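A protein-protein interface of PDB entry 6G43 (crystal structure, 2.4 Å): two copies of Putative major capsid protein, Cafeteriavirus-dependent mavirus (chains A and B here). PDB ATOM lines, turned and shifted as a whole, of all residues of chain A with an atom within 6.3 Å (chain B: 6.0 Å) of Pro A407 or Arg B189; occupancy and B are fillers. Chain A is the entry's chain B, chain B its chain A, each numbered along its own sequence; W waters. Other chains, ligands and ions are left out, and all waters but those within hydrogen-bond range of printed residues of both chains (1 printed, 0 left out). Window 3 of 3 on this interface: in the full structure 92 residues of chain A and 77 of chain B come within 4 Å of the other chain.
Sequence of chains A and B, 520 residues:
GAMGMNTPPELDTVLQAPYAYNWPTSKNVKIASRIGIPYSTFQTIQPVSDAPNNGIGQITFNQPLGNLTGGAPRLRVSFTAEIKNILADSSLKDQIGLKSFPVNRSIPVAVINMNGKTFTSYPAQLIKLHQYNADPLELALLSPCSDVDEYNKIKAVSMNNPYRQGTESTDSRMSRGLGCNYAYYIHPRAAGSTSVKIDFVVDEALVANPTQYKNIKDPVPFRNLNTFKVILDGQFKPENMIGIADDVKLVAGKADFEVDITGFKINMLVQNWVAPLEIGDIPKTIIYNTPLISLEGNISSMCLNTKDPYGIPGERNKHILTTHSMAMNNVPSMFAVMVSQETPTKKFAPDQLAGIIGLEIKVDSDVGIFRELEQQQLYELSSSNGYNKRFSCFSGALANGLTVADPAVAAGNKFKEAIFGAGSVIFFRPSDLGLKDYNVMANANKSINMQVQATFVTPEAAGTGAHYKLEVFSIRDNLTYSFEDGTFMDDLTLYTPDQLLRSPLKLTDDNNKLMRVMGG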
ATOM      1  N   LEU A 402      -1.281  26.775  18.493  1.00  0.00           N
ATOM      2  CA  LEU A 402      -1.415  26.745  19.959  1.00  0.00           C
ATOM      3  C   LEU A 402      -2.175  25.511  20.441  1.00  0.00           C
ATOM      4  O   LEU A 402      -1.790  24.898  21.437  1.00  0.00           O
ATOM      5  CB  LEU A 402      -2.089  28.019  20.479  1.00  0.00           C
ATOM      6  CG  LEU A 402      -1.284  29.298  20.234  1.00  0.00           C
ATOM      7  CD1 LEU A 402      -2.156  30.545  20.262  1.00  0.00           C
ATOM      8  CD2 LEU A 402      -0.139  29.414  21.232  1.00  0.00           C
ATOM      9  N   VAL A 404      -2.219  22.642  18.908  1.00  0.00           N
ATOM     10  CA  VAL A 404      -1.342  21.487  18.666  1.00  0.00           C
ATOM     11  C   VAL A 404      -0.162  21.455  19.636  1.00  0.00           C
ATOM     12  O   VAL A 404       0.182  20.393  20.155  1.00  0.00           O
ATOM     13  CB  VAL A 404      -0.808  21.471  17.214  1.00  0.00           C
ATOM     14  CG1 VAL A 404       0.140  20.297  16.986  1.00  0.00           C
ATOM     15  CG2 VAL A 404      -1.962  21.390  16.225  1.00  0.00           C
ATOM     16  N   ALA A 405       0.465  22.610  19.852  1.00  0.00           N
ATOM     17  CA  ALA A 405       1.617  22.732  20.753  1.00  0.00           C
ATOM     18  C   ALA A 405       1.278  22.534  22.236  1.00  0.00           C
ATOM     19  O   ALA A 405       2.175  22.274  23.041  1.00  0.00           O
ATOM     20  CB  ALA A 405       2.297  24.077  20.550  1.00  0.00           C
ATOM     21  N   ASP A 406       0.000  22.681  22.590  1.00  0.00           N
ATOM     22  CA  ASP A 406      -0.514  22.383  23.930  1.00  0.00           C
ATOM     23  C   ASP A 406       0.048  21.050  24.466  1.00  0.00           C
ATOM     24  O   ASP A 406      -0.154  20.008  23.836  1.00  0.00           O
ATOM     25  CB  ASP A 406      -2.049  22.329  23.869  1.00  0.00           C
ATOM     26  CG  ASP A 406      -2.708  22.160  25.238  1.00  0.00           C
ATOM     27  OD1 ASP A 406      -2.031  22.273  26.283  1.00  0.00           O
ATOM     28  OD2 ASP A 406      -3.935  21.920  25.265  1.00  0.00           O
ATOM     29  N   PRO A 407       0.769  21.080  25.612  1.00  0.00           N
ATOM     30  CA  PRO A 407       1.350  19.833  26.152  1.00  0.00           C
ATOM     31  C   PRO A 407       0.329  18.770  26.596  1.00  0.00           C
ATOM     32  O   PRO A 407       0.675  17.587  26.658  1.00  0.00           O
ATOM     33  CB  PRO A 407       2.191  20.316  27.345  1.00  0.00           C
ATOM     34  CG  PRO A 407       1.606  21.634  27.720  1.00  0.00           C
ATOM     35  CD  PRO A 407       1.169  22.249  26.422  1.00  0.00           C
ATOM     36  N   ALA A 408      -0.902  19.190  26.898  1.00  0.00           N
ATOM     37  CA  ALA A 408      -2.021  18.274  27.157  1.00  0.00           C
ATOM     38  C   ALA A 408      -2.308  17.305  25.993  1.00  0.00           C
ATOM     39  O   ALA A 408      -2.770  16.187  26.218  1.00  0.00           O
ATOM     40  CB  ALA A 408      -3.274  19.072  27.493  1.00  0.00           C
ATOM     41  N   VAL A 409      -2.041  17.748  24.763  1.00  0.00           N
ATOM     42  CA  VAL A 409      -2.132  16.891  23.579  1.00  0.00           C
ATOM     43  C   VAL A 409      -0.848  16.068  23.478  1.00  0.00           C
ATOM     44  O   VAL A 409       0.243  16.632  23.356  1.00  0.00           O
ATOM     45  CB  VAL A 409      -2.313  17.716  22.285  1.00  0.00           C
ATOM     46  CG1 VAL A 409      -2.435  16.802  21.072  1.00  0.00           C
ATOM     47  CG2 VAL A 409      -3.539  18.615  22.380  1.00  0.00           C
ATOM     48  N   ALA A 410      -0.982  14.743  23.525  1.00  0.00           N
ATOM     49  CA  ALA A 410       0.165  13.833  23.436  1.00  0.00           C
ATOM     50  C   ALA A 410       0.761  13.809  22.031  1.00  0.00           C
ATOM     51  O   ALA A 410       0.123  14.241  21.066  1.00  0.00           O
ATOM     52  CB  ALA A 410      -0.241  12.429  23.853  1.00  0.00           C
ATOM     53  N   LYS A 414      -0.945  14.685  17.836  1.00  0.00           N
ATOM     54  CA  LYS A 414      -0.595  15.995  17.275  1.00  0.00           C
ATOM     55  C   LYS A 414      -1.212  16.199  15.896  1.00  0.00           C
ATOM     56  O   LYS A 414      -1.850  17.224  15.641  1.00  0.00           O
ATOM     57  CB  LYS A 414       0.926  16.144  17.158  1.00  0.00           C
ATOM     58  CG  LYS A 414       1.683  16.183  18.478  1.00  0.00           C
ATOM     59  CD  LYS A 414       1.421  17.459  19.261  1.00  0.00           C
ATOM     60  CE  LYS A 414       2.401  17.604  20.415  1.00  0.00           C
ATOM     61  NZ  LYS A 414       1.997  18.673  21.370  1.00  0.00           N
ATOM     62  N   ILE B  86       4.282  32.250  32.701  1.00  0.00           N
ATOM     63  CA  ILE B  86       2.981  31.645  32.384  1.00  0.00           C
ATOM     64  C   ILE B  86       2.754  30.493  33.361  1.00  0.00           C
ATOM     65  O   ILE B  86       3.669  29.711  33.610  1.00  0.00           O
ATOM     66  CB  ILE B  86       2.926  31.115  30.929  1.00  0.00           C
ATOM     67  CG1 ILE B  86       3.246  32.241  29.932  1.00  0.00           C
ATOM     68  CG2 ILE B  86       1.551  30.524  30.611  1.00  0.00           C
ATOM     69  CD1 ILE B  86       3.421  31.781  28.499  1.00  0.00           C
ATOM     70  N   LEU B  87       1.542  30.379  33.904  1.00  0.00           N
ATOM     71  CA  LEU B  87       1.213  29.285  34.823  1.00  0.00           C
ATOM     72  C   LEU B  87       1.441  27.937  34.142  1.00  0.00           C
ATOM     73  O   LEU B  87       1.138  27.774  32.954  1.00  0.00           O
ATOM     74  CB  LEU B  87      -0.237  29.385  35.311  1.00  0.00           C
ATOM     75  CG  LEU B  87      -0.687  28.356  36.362  1.00  0.00           C
ATOM     76  CD1 LEU B  87       0.050  28.560  37.679  1.00  0.00           C
ATOM     77  CD2 LEU B  87      -2.193  28.428  36.582  1.00  0.00           C
ATOM     78  N   ASP B  89       1.393  24.375  32.560  1.00  0.00           N
ATOM     79  CA  ASP B  89       0.388  23.613  31.798  1.00  0.00           C
ATOM     80  C   ASP B  89      -0.845  24.435  31.378  1.00  0.00           C
ATOM     81  O   ASP B  89      -1.965  23.916  31.324  1.00  0.00           O
ATOM     82  CB  ASP B  89      -0.024  22.335  32.557  1.00  0.00           C
ATOM     83  CG  ASP B  89       1.171  21.478  32.963  1.00  0.00           C
ATOM     84  OD1 ASP B  89       2.137  21.365  32.170  1.00  0.00           O
ATOM     85  OD2 ASP B  89       1.139  20.913  34.079  1.00  0.00           O
ATOM     86  N   SER B  90      -0.625  25.714  31.072  1.00  0.00           N
ATOM     87  CA  SER B  90      -1.637  26.550  30.436  1.00  0.00           C
ATOM     88  C   SER B  90      -1.686  26.176  28.958  1.00  0.00           C
ATOM     89  O   SER B  90      -0.643  26.112  28.304  1.00  0.00           O
ATOM     90  CB  SER B  90      -1.278  28.028  30.586  1.00  0.00           C
ATOM     91  OG  SER B  90      -1.291  28.423  31.945  1.00  0.00           O
ATOM     92  N   SER B  91      -2.885  25.915  28.440  1.00  0.00           N
ATOM     93  CA  SER B  91      -3.054  25.528  27.034  1.00  0.00           C
ATOM     94  C   SER B  91      -2.680  26.650  26.058  1.00  0.00           C
ATOM     95  O   SER B  91      -2.148  26.383  24.976  1.00  0.00           O
ATOM     96  CB  SER B  91      -4.495  25.075  26.772  1.00  0.00           C
ATOM     97  OG  SER B  91      -5.399  26.167  26.801  1.00  0.00           O
ATOM     98  N   LEU B  92      -2.968  27.890  26.462  1.00  0.00           N
ATOM     99  CA  LEU B  92      -2.762  29.095  25.650  1.00  0.00           C
ATOM    100  C   LEU B  92      -3.574  29.115  24.344  1.00  0.00           C
ATOM    101  O   LEU B  92      -3.183  29.782  23.388  1.00  0.00           O
ATOM    102  CB  LEU B  92      -1.264  29.333  25.374  1.00  0.00           C
ATOM    103  CG  LEU B  92      -0.354  29.448  26.596  1.00  0.00           C
ATOM    104  CD1 LEU B  92       1.096  29.568  26.158  1.00  0.00           C
ATOM    105  CD2 LEU B  92      -0.747  30.639  27.458  1.00  0.00           C
ATOM    106  N   ILE B 186       5.769  27.955  16.948  1.00  0.00           N
ATOM    107  CA  ILE B 186       5.854  27.783  18.398  1.00  0.00           C
ATOM    108  C   ILE B 186       6.847  26.659  18.695  1.00  0.00           C
ATOM    109  O   ILE B 186       6.712  25.554  18.161  1.00  0.00           O
ATOM    110  CB  ILE B 186       4.479  27.418  18.997  1.00  0.00           C
ATOM    111  CG1 ILE B 186       3.420  28.457  18.610  1.00  0.00           C
ATOM    112  CG2 ILE B 186       4.547  27.334  20.519  1.00  0.00           C
ATOM    113  CD1 ILE B 186       2.025  27.887  18.564  1.00  0.00           C
ATOM    114  N   HIS B 187       7.834  26.942  19.544  1.00  0.00           N
ATOM    115  CA  HIS B 187       8.825  25.944  19.950  1.00  0.00           C
ATOM    116  C   HIS B 187       8.147  24.891  20.839  1.00  0.00           C
ATOM    117  O   HIS B 187       7.198  25.223  21.555  1.00  0.00           O
ATOM    118  CB  HIS B 187       9.970  26.603  20.726  1.00  0.00           C
ATOM    119  CG  HIS B 187      10.865  27.467  19.891  1.00  0.00           C
ATOM    120  ND1 HIS B 187      12.239  27.380  19.946  1.00  0.00           N
ATOM    121  CD2 HIS B 187      10.587  28.442  18.992  1.00  0.00           C
ATOM    122  CE1 HIS B 187      12.770  28.262  19.116  1.00  0.00           C
ATOM    123  NE2 HIS B 187      11.789  28.919  18.526  1.00  0.00           N
ATOM    124  N   PRO B 188       8.625  23.626  20.803  1.00  0.00           N
ATOM    125  CA  PRO B 188       8.002  22.581  21.632  1.00  0.00           C
ATOM    126  C   PRO B 188       7.919  22.957  23.118  1.00  0.00           C
ATOM    127  O   PRO B 188       8.892  23.464  23.681  1.00  0.00           O
ATOM    128  CB  PRO B 188       8.924  21.372  21.434  1.00  0.00           C
ATOM    129  CG  PRO B 188       9.578  21.603  20.116  1.00  0.00           C
ATOM    130  CD  PRO B 188       9.744  23.090  20.003  1.00  0.00           C
ATOM    131  N   ARG B 189       6.753  22.727  23.716  1.00  0.00           N
ATOM    132  CA  ARG B 189       6.503  23.040  25.118  1.00  0.00           C
ATOM    133  C   ARG B 189       6.502  21.753  25.935  1.00  0.00           C
ATOM    134  O   ARG B 189       5.670  20.869  25.707  1.00  0.00           O
ATOM    135  CB  ARG B 189       5.148  23.729  25.271  1.00  0.00           C
ATOM    136  CG  ARG B 189       5.007  25.033  24.503  1.00  0.00           C
ATOM    137  CD  ARG B 189       3.599  25.585  24.655  1.00  0.00           C
ATOM    138  NE  ARG B 189       3.300  25.917  26.049  1.00  0.00           N
ATOM    139  CZ  ARG B 189       2.085  26.143  26.550  1.00  0.00           C
ATOM    140  NH1 ARG B 189       0.990  26.084  25.788  1.00  0.00           N
ATOM    141  NH2 ARG B 189       1.961  26.433  27.844  1.00  0.00           N
ATOM    142  N   ALA B 190       7.438  21.651  26.876  1.00  0.00           N
ATOM    143  CA  ALA B 190       7.512  20.504  27.778  1.00  0.00           C
ATOM    144  C   ALA B 190       6.415  20.595  28.837  1.00  0.00           C
ATOM    145  O   ALA B 190       5.934  21.689  29.154  1.00  0.00           O
ATOM    146  CB  ALA B 190       8.882  20.443  28.438  1.00  0.00           C
ATOM    147  N   ALA B 191       6.023  19.444  29.377  1.00  0.00           N
ATOM    148  CA  ALA B 191       5.045  19.389  30.463  1.00  0.00           C
ATOM    149  C   ALA B 191       5.634  20.053  31.708  1.00  0.00           C
ATOM    150  O   ALA B 191       6.768  19.760  32.095  1.00  0.00           O
ATOM    151  CB  ALA B 191       4.659  17.948  30.758  1.00  0.00           C
ATOM    152  N   GLY B 192       4.870  20.969  32.301  1.00  0.00           N
ATOM    153  CA  GLY B 192       5.320  21.748  33.460  1.00  0.00           C
ATOM    154  C   GLY B 192       6.074  23.036  33.158  1.00  0.00           C
ATOM    155  O   GLY B 192       6.461  23.749  34.087  1.00  0.00           O
ATOM    156  N   SER B 193       6.282  23.350  31.877  1.00  0.00           N
ATOM    157  CA  SER B 193       7.017  24.556  31.485  1.00  0.00           C
ATOM    158  C   SER B 193       6.186  25.818  31.733  1.00  0.00           C
ATOM    159  O   SER B 193       4.974  25.826  31.502  1.00  0.00           O
ATOM    160  CB  SER B 193       7.425  24.482  30.011  1.00  0.00           C
ATOM    161  OG  SER B 193       6.289  24.366  29.170  1.00  0.00           O
ATOM    162  N   SER B 195       7.214  28.859  30.393  1.00  0.00           N
ATOM    163  CA  SER B 195       7.548  29.782  29.314  1.00  0.00           C
ATOM    164  C   SER B 195       7.356  29.145  27.946  1.00  0.00           C
ATOM    165  O   SER B 195       7.241  27.924  27.822  1.00  0.00           O
ATOM    166  CB  SER B 195       8.987  30.281  29.458  1.00  0.00           C
ATOM    167  OG  SER B 195       9.910  29.212  29.350  1.00  0.00           O
ATOM    168  N   VAL B 196       7.332  29.995  26.924  1.00  0.00           N
ATOM    169  CA  VAL B 196       7.142  29.565  25.543  1.00  0.00           C
ATOM    170  C   VAL B 196       7.918  30.493  24.609  1.00  0.00           C
ATOM    171  O   VAL B 196       8.012  31.698  24.860  1.00  0.00           O
ATOM    172  CB  VAL B 196       5.636  29.512  25.172  1.00  0.00           C
ATOM    173  CG1 VAL B 196       4.998  30.898  25.181  1.00  0.00           C
ATOM    174  CG2 VAL B 196       5.429  28.825  23.828  1.00  0.00           C
HETATM  175  O   HOH W   1      -0.043  25.975  23.214  1.00  0.00           O
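No position is printed for both chains. Of the 7 pairs that touch across the chains among the printed residues, none has its exchanged pair printed and touching as well.
Water W1 lies within hydrogen-bond range of O of Leu A402 (2.7 Å), O of Ser B91 (2.8 Å), NH1 of Arg B189 (2.8 Å) and N of Asp A406 (3.4 Å).
Of chain B, only Arg B189 (3.9 Å) comes within 4 Å of Pro A407. Arg B189 touches just these residues of chain A: Ala A405 and Pro A407. Printed residues of chain B within 4 Å of Asp A406: Ser B91 (3.5 Å). Of the printed residues of chain B, Ala A405 touches Ile B186 (3.96 Å) and Arg B189 (3.9 Å).
The backbone carbonyl oxygen (O) of Ser B91 sits at hydrogen-bond distance from the guanidinium group (NH1) of Arg B189, 3.3 Å away. NH2 of Arg B189 lies within hydrogen-bond range of O of Ser B90 (2.7 Å). The side-chain carboxylate (OD1) of Asp A406 lies close to the backbone NH (N) of Ala A408, at 3.3 Å.
Of the 16 printed residues of chain B, 4 touch a printed residue of chain A. Hydrophobic or aromatic side chains of chain B within 4 Å of the printed part of chain A: Ile B186. Printed residues of chain A that touch a printed residue of chain B: Leu A402, Ala A405, Asp A406 and Pro A407. Along chain A the printed residues that touch a printed residue of chain B span positions 402 to 407.
Leu A402 touches Ser B91 (O to O, 3.9 Å). Leu B92 touches Leu A402 (O to CD1, 3.4 Å). Leu A402 touches Ile B186. Ala A405 touches Ile B186. Arg B189 touches Ala A405 (CD to O, 3.9 Å). Asp A406 touches Ser B91 (OD1 to CA, 3.5 Å). Arg B189 touches Pro A407.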
